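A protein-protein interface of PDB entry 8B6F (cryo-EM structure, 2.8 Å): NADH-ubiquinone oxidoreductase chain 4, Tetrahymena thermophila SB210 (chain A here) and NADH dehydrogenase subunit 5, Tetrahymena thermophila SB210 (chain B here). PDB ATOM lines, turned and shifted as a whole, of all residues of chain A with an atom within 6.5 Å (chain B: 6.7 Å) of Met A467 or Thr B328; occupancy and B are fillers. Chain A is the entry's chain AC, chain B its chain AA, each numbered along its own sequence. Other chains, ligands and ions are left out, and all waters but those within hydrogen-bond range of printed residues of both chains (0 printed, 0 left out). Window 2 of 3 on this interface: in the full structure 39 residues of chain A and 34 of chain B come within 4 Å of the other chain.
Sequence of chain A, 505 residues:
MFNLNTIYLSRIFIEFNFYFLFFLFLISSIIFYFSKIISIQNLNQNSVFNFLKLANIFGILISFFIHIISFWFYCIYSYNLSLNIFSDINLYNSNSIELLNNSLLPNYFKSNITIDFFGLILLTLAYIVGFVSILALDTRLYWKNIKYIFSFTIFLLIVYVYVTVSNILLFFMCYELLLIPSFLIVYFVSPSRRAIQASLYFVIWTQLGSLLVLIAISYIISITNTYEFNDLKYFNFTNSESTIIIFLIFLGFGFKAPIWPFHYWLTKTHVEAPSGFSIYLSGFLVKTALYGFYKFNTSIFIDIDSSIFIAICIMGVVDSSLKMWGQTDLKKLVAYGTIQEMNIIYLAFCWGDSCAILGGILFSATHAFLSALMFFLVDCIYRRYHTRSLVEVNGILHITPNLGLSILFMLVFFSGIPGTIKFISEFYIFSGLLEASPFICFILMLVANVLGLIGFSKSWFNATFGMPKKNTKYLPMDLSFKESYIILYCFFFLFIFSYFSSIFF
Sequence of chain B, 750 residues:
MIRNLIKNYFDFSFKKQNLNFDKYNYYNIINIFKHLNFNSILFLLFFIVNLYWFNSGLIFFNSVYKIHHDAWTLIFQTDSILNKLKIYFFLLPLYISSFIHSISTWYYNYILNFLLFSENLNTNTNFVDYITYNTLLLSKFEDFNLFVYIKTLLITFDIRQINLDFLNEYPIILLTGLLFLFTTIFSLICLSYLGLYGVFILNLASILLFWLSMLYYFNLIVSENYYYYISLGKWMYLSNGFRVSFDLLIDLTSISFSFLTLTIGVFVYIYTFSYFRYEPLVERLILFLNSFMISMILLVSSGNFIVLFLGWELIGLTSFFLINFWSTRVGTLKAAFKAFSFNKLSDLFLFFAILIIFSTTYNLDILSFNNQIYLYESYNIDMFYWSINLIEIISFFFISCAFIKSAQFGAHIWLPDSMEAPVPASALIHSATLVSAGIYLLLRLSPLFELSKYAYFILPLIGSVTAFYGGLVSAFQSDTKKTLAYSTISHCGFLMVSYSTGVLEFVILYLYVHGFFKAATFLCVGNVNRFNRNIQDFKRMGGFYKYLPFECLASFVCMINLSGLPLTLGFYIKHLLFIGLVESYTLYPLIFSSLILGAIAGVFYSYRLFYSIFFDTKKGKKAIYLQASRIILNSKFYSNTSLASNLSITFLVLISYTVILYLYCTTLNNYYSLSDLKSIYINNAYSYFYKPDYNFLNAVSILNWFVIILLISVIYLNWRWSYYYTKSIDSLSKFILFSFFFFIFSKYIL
NE2 of His A398 touches CG2 of Thr B328, at 3.4 Å. Asn B324 touches Phe A465 (ND2 to CE2, 3.1 Å). Phe A465 touches Ser B327 (CD1 to CB, 3.5 Å). Gly A466 touches Val B330. O of Thr B328 touches N of Met A467, at 3.8 Å.
The side-chain hydroxyl (OG) of Ser B327 sits at hydrogen-bond distance from a ring nitrogen (NE2) of His A398, at 2.9 Å. The backbone NH of Gly A466 sits at hydrogen-bond distance from the backbone carbonyl oxygen of Ser B327 (3.2 Å). The backbone carbonyl oxygen (O) of Gly A466 sits close to the backbone carbonyl oxygen (O) of Thr B328, at 3.2 Å.
Printed residues of chain A that touch a printed residue of chain B: His A398, Phe A465, Gly A466 and Met A467. Among the printed residues, 8 pairs touch across the chains.
The side-chain amide nitrogen (ND2) of Asn A394 is in hydrogen-bond range of the backbone carbonyl oxygen (O) of Phe A465 (2.9 Å). The side-chain amide oxygen of Asn A394 lies within hydrogen-bond range of the backbone NH of Met A467 (3.1 Å). O of Phe A465 is in hydrogen-bond range of N of Gly A395, at 3.0 Å. O of Gly A466 sits close to ND1 of His A398, 3.2 Å away.
Printed residues of chain B within 4 Å of Gly A466: Ser B327 (3.2 Å), Thr B328 (3.2 Å) and Val B330 (3.9 Å). Printed residues of chain B within 4 Å of Met A467: Thr B328. Lys A469 touches none of the printed residues of chain B. Of the printed residues of chain A, Ser B327 touches His A398 (2.9 Å), Phe A465 (3.5 Å) and Gly A466 (3.2 Å). Thr B328 touches three residues of chain A. Of the printed residues of chain A, Val B330 touches Gly A466. The nearest residue of chain A that does not touch Thr B328 is Phe A465 (5.4 Å).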
ATOM      1  N   ASN A 394      -4.623 -25.808 -14.603  1.00  0.00           N
ATOM      2  CA  ASN A 394      -6.012 -25.960 -14.996  1.00  0.00           C
ATOM      3  C   ASN A 394      -6.701 -26.892 -14.011  1.00  0.00           C
ATOM      4  O   ASN A 394      -6.084 -27.820 -13.482  1.00  0.00           O
ATOM      5  CB  ASN A 394      -6.116 -26.498 -16.428  1.00  0.00           C
ATOM      6  CG  ASN A 394      -7.545 -26.651 -16.890  1.00  0.00           C
ATOM      7  OD1 ASN A 394      -8.058 -27.762 -17.005  1.00  0.00           O
ATOM      8  ND2 ASN A 394      -8.203 -25.528 -17.151  1.00  0.00           N
ATOM      9  N   GLY A 395      -7.980 -26.631 -13.767  1.00  0.00           N
ATOM     10  CA  GLY A 395      -8.766 -27.480 -12.886  1.00  0.00           C
ATOM     11  C   GLY A 395      -8.332 -27.463 -11.437  1.00  0.00           C
ATOM     12  O   GLY A 395      -8.277 -28.521 -10.799  1.00  0.00           O
ATOM     13  N   HIS A 398     -10.865 -28.993  -8.594  1.00  0.00           N
ATOM     14  CA  HIS A 398     -11.148 -30.414  -8.441  1.00  0.00           C
ATOM     15  C   HIS A 398     -10.080 -31.164  -7.659  1.00  0.00           C
ATOM     16  O   HIS A 398     -10.306 -32.325  -7.302  1.00  0.00           O
ATOM     17  CB  HIS A 398     -11.324 -31.054  -9.818  1.00  0.00           C
ATOM     18  CG  HIS A 398     -12.386 -30.403 -10.647  1.00  0.00           C
ATOM     19  ND1 HIS A 398     -12.138 -29.304 -11.441  1.00  0.00           N
ATOM     20  CD2 HIS A 398     -13.702 -30.680 -10.788  1.00  0.00           C
ATOM     21  CE1 HIS A 398     -13.256 -28.938 -12.042  1.00  0.00           C
ATOM     22  NE2 HIS A 398     -14.220 -29.757 -11.663  1.00  0.00           N
ATOM     23  N   PHE A 465     -11.561 -23.957 -13.225  1.00  0.00           N
ATOM     24  CA  PHE A 465     -12.326 -25.047 -13.808  1.00  0.00           C
ATOM     25  C   PHE A 465     -11.488 -25.802 -14.832  1.00  0.00           C
ATOM     26  O   PHE A 465     -10.379 -25.402 -15.190  1.00  0.00           O
ATOM     27  CB  PHE A 465     -13.611 -24.513 -14.447  1.00  0.00           C
ATOM     28  CG  PHE A 465     -14.469 -23.734 -13.497  1.00  0.00           C
ATOM     29  CD1 PHE A 465     -15.107 -24.367 -12.445  1.00  0.00           C
ATOM     30  CD2 PHE A 465     -14.638 -22.371 -13.655  1.00  0.00           C
ATOM     31  CE1 PHE A 465     -15.895 -23.655 -11.566  1.00  0.00           C
ATOM     32  CE2 PHE A 465     -15.425 -21.652 -12.780  1.00  0.00           C
ATOM     33  CZ  PHE A 465     -16.054 -22.296 -11.733  1.00  0.00           C
ATOM     34  N   GLY A 466     -12.041 -26.914 -15.303  1.00  0.00           N
ATOM     35  CA  GLY A 466     -11.322 -27.805 -16.189  1.00  0.00           C
ATOM     36  C   GLY A 466     -11.128 -29.168 -15.560  1.00  0.00           C
ATOM     37  O   GLY A 466     -11.877 -29.549 -14.659  1.00  0.00           O
ATOM     38  N   MET A 467     -10.119 -29.905 -16.011  1.00  0.00           N
ATOM     39  CA  MET A 467      -9.897 -31.259 -15.523  1.00  0.00           C
ATOM     40  C   MET A 467      -8.401 -31.534 -15.414  1.00  0.00           C
ATOM     41  O   MET A 467      -7.731 -31.705 -16.439  1.00  0.00           O
ATOM     42  CB  MET A 467     -10.572 -32.260 -16.458  1.00  0.00           C
ATOM     43  CG  MET A 467     -10.768 -33.639 -15.868  1.00  0.00           C
ATOM     44  SD  MET A 467     -12.317 -34.390 -16.398  1.00  0.00           S
ATOM     45  CE  MET A 467     -12.237 -34.143 -18.169  1.00  0.00           C
ATOM     46  N   PRO A 468      -7.837 -31.585 -14.199  1.00  0.00           N
ATOM     47  CA  PRO A 468      -6.372 -31.748 -14.059  1.00  0.00           C
ATOM     48  C   PRO A 468      -5.897 -33.185 -14.262  1.00  0.00           C
ATOM     49  O   PRO A 468      -5.650 -33.948 -13.330  1.00  0.00           O
ATOM     50  CB  PRO A 468      -6.120 -31.260 -12.633  1.00  0.00           C
ATOM     51  CG  PRO A 468      -7.367 -31.607 -11.903  1.00  0.00           C
ATOM     52  CD  PRO A 468      -8.500 -31.477 -12.887  1.00  0.00           C
ATOM     53  N   LYS A 469      -5.764 -33.568 -15.529  1.00  0.00           N
ATOM     54  CA  LYS A 469      -5.308 -34.899 -15.901  1.00  0.00           C
ATOM     55  C   LYS A 469      -3.790 -35.011 -15.976  1.00  0.00           C
ATOM     56  O   LYS A 469      -3.269 -36.128 -16.031  1.00  0.00           O
ATOM     57  CB  LYS A 469      -5.920 -35.290 -17.254  1.00  0.00           C
ATOM     58  CG  LYS A 469      -5.562 -36.684 -17.754  1.00  0.00           C
ATOM     59  CD  LYS A 469      -6.020 -37.764 -16.792  1.00  0.00           C
ATOM     60  CE  LYS A 469      -5.682 -39.144 -17.320  1.00  0.00           C
ATOM     61  NZ  LYS A 469      -6.275 -40.209 -16.469  1.00  0.00           N
ATOM     62  N   LYS A 470      -3.073 -33.892 -15.955  1.00  0.00           N
ATOM     63  CA  LYS A 470      -1.635 -33.885 -16.175  1.00  0.00           C
ATOM     64  C   LYS A 470      -0.879 -34.010 -14.858  1.00  0.00           C
ATOM     65  O   LYS A 470      -1.250 -33.393 -13.855  1.00  0.00           O
ATOM     66  CB  LYS A 470      -1.221 -32.601 -16.895  1.00  0.00           C
ATOM     67  CG  LYS A 470       0.247 -32.546 -17.279  1.00  0.00           C
ATOM     68  CD  LYS A 470       0.606 -31.225 -17.944  1.00  0.00           C
ATOM     69  CE  LYS A 470       0.500 -30.060 -16.973  1.00  0.00           C
ATOM     70  NZ  LYS A 470       1.021 -28.797 -17.566  1.00  0.00           N
ATOM     71  N   ASN B 324     -22.604 -23.569 -15.029  1.00  0.00           N
ATOM     72  CA  ASN B 324     -21.285 -24.180 -14.981  1.00  0.00           C
ATOM     73  C   ASN B 324     -21.221 -25.348 -14.006  1.00  0.00           C
ATOM     74  O   ASN B 324     -20.128 -25.710 -13.561  1.00  0.00           O
ATOM     75  CB  ASN B 324     -20.240 -23.128 -14.607  1.00  0.00           C
ATOM     76  CG  ASN B 324     -18.832 -23.561 -14.942  1.00  0.00           C
ATOM     77  OD1 ASN B 324     -18.620 -24.399 -15.815  1.00  0.00           O
ATOM     78  ND2 ASN B 324     -17.858 -22.992 -14.246  1.00  0.00           N
ATOM     79  N   PHE B 325     -22.367 -25.937 -13.656  1.00  0.00           N
ATOM     80  CA  PHE B 325     -22.363 -27.066 -12.733  1.00  0.00           C
ATOM     81  C   PHE B 325     -21.384 -28.150 -13.163  1.00  0.00           C
ATOM     82  O   PHE B 325     -20.646 -28.693 -12.335  1.00  0.00           O
ATOM     83  CB  PHE B 325     -23.772 -27.643 -12.606  1.00  0.00           C
ATOM     84  CG  PHE B 325     -23.878 -28.741 -11.595  1.00  0.00           C
ATOM     85  CD1 PHE B 325     -24.046 -28.444 -10.254  1.00  0.00           C
ATOM     86  CD2 PHE B 325     -23.808 -30.066 -11.981  1.00  0.00           C
ATOM     87  CE1 PHE B 325     -24.138 -29.449  -9.315  1.00  0.00           C
ATOM     88  CE2 PHE B 325     -23.899 -31.077 -11.047  1.00  0.00           C
ATOM     89  CZ  PHE B 325     -24.066 -30.769  -9.713  1.00  0.00           C
ATOM     90  N   TRP B 326     -21.360 -28.482 -14.455  1.00  0.00           N
ATOM     91  CA  TRP B 326     -20.402 -29.457 -14.978  1.00  0.00           C
ATOM     92  C   TRP B 326     -19.041 -28.774 -15.116  1.00  0.00           C
ATOM     93  O   TRP B 326     -18.542 -28.499 -16.209  1.00  0.00           O
ATOM     94  CB  TRP B 326     -20.889 -30.029 -16.303  1.00  0.00           C
ATOM     95  CG  TRP B 326     -22.224 -30.708 -16.209  1.00  0.00           C
ATOM     96  CD1 TRP B 326     -23.396 -30.290 -16.769  1.00  0.00           C
ATOM     97  CD2 TRP B 326     -22.526 -31.922 -15.510  1.00  0.00           C
ATOM     98  NE1 TRP B 326     -24.407 -31.168 -16.465  1.00  0.00           N
ATOM     99  CE2 TRP B 326     -23.899 -32.179 -15.693  1.00  0.00           C
ATOM    100  CE3 TRP B 326     -21.768 -32.817 -14.747  1.00  0.00           C
ATOM    101  CZ2 TRP B 326     -24.529 -33.292 -15.143  1.00  0.00           C
ATOM    102  CZ3 TRP B 326     -22.395 -33.921 -14.202  1.00  0.00           C
ATOM    103  CH2 TRP B 326     -23.763 -34.151 -14.404  1.00  0.00           C
ATOM    104  N   SER B 327     -18.431 -28.506 -13.960  1.00  0.00           N
ATOM    105  CA  SER B 327     -17.197 -27.728 -13.928  1.00  0.00           C
ATOM    106  C   SER B 327     -16.036 -28.448 -14.604  1.00  0.00           C
ATOM    107  O   SER B 327     -15.107 -27.794 -15.089  1.00  0.00           O
ATOM    108  CB  SER B 327     -16.838 -27.391 -12.483  1.00  0.00           C
ATOM    109  OG  SER B 327     -16.889 -28.546 -11.662  1.00  0.00           O
ATOM    110  N   THR B 328     -16.058 -29.781 -14.642  1.00  0.00           N
ATOM    111  CA  THR B 328     -14.950 -30.513 -15.245  1.00  0.00           C
ATOM    112  C   THR B 328     -14.819 -30.194 -16.726  1.00  0.00           C
ATOM    113  O   THR B 328     -13.705 -30.106 -17.254  1.00  0.00           O
ATOM    114  CB  THR B 328     -15.133 -32.015 -15.052  1.00  0.00           C
ATOM    115  OG1 THR B 328     -16.393 -32.410 -15.599  1.00  0.00           O
ATOM    116  CG2 THR B 328     -15.086 -32.377 -13.578  1.00  0.00           C
ATOM    117  N   ARG B 329     -15.944 -30.026 -17.415  1.00  0.00           N
ATOM    118  CA  ARG B 329     -15.921 -29.714 -18.835  1.00  0.00           C
ATOM    119  C   ARG B 329     -15.700 -28.226 -19.054  1.00  0.00           C
ATOM    120  O   ARG B 329     -16.306 -27.386 -18.383  1.00  0.00           O
ATOM    121  CB  ARG B 329     -17.233 -30.136 -19.496  1.00  0.00           C
ATOM    122  CG  ARG B 329     -17.374 -31.629 -19.717  1.00  0.00           C
ATOM    123  CD  ARG B 329     -18.753 -31.980 -20.252  1.00  0.00           C
ATOM    124  NE  ARG B 329     -19.191 -31.054 -21.291  1.00  0.00           N
ATOM    125  CZ  ARG B 329     -18.809 -31.108 -22.559  1.00  0.00           C
ATOM    126  NH1 ARG B 329     -17.966 -32.033 -22.989  1.00  0.00           N
ATOM    127  NH2 ARG B 329     -19.285 -30.212 -23.418  1.00  0.00           N
ATOM    128  N   VAL B 330     -14.821 -27.904 -20.002  1.00  0.00           N
ATOM    129  CA  VAL B 330     -14.613 -26.515 -20.391  1.00  0.00           C
ATOM    130  C   VAL B 330     -15.615 -26.053 -21.441  1.00  0.00           C
ATOM    131  O   VAL B 330     -15.771 -24.841 -21.641  1.00  0.00           O
ATOM    132  CB  VAL B 330     -13.183 -26.287 -20.910  1.00  0.00           C
ATOM    133  CG1 VAL B 330     -12.184 -26.440 -19.777  1.00  0.00           C
ATOM    134  CG2 VAL B 330     -12.858 -27.236 -22.059  1.00  0.00           C
ATOM    135  N   GLY B 331     -16.290 -26.978 -22.123  1.00  0.00           N
ATOM    136  CA  GLY B 331     -17.359 -26.575 -23.019  1.00  0.00           C
ATOM    137  C   GLY B 331     -18.497 -25.908 -22.274  1.00  0.00           C
ATOM    138  O   GLY B 331     -19.068 -24.921 -22.744  1.00  0.00           O
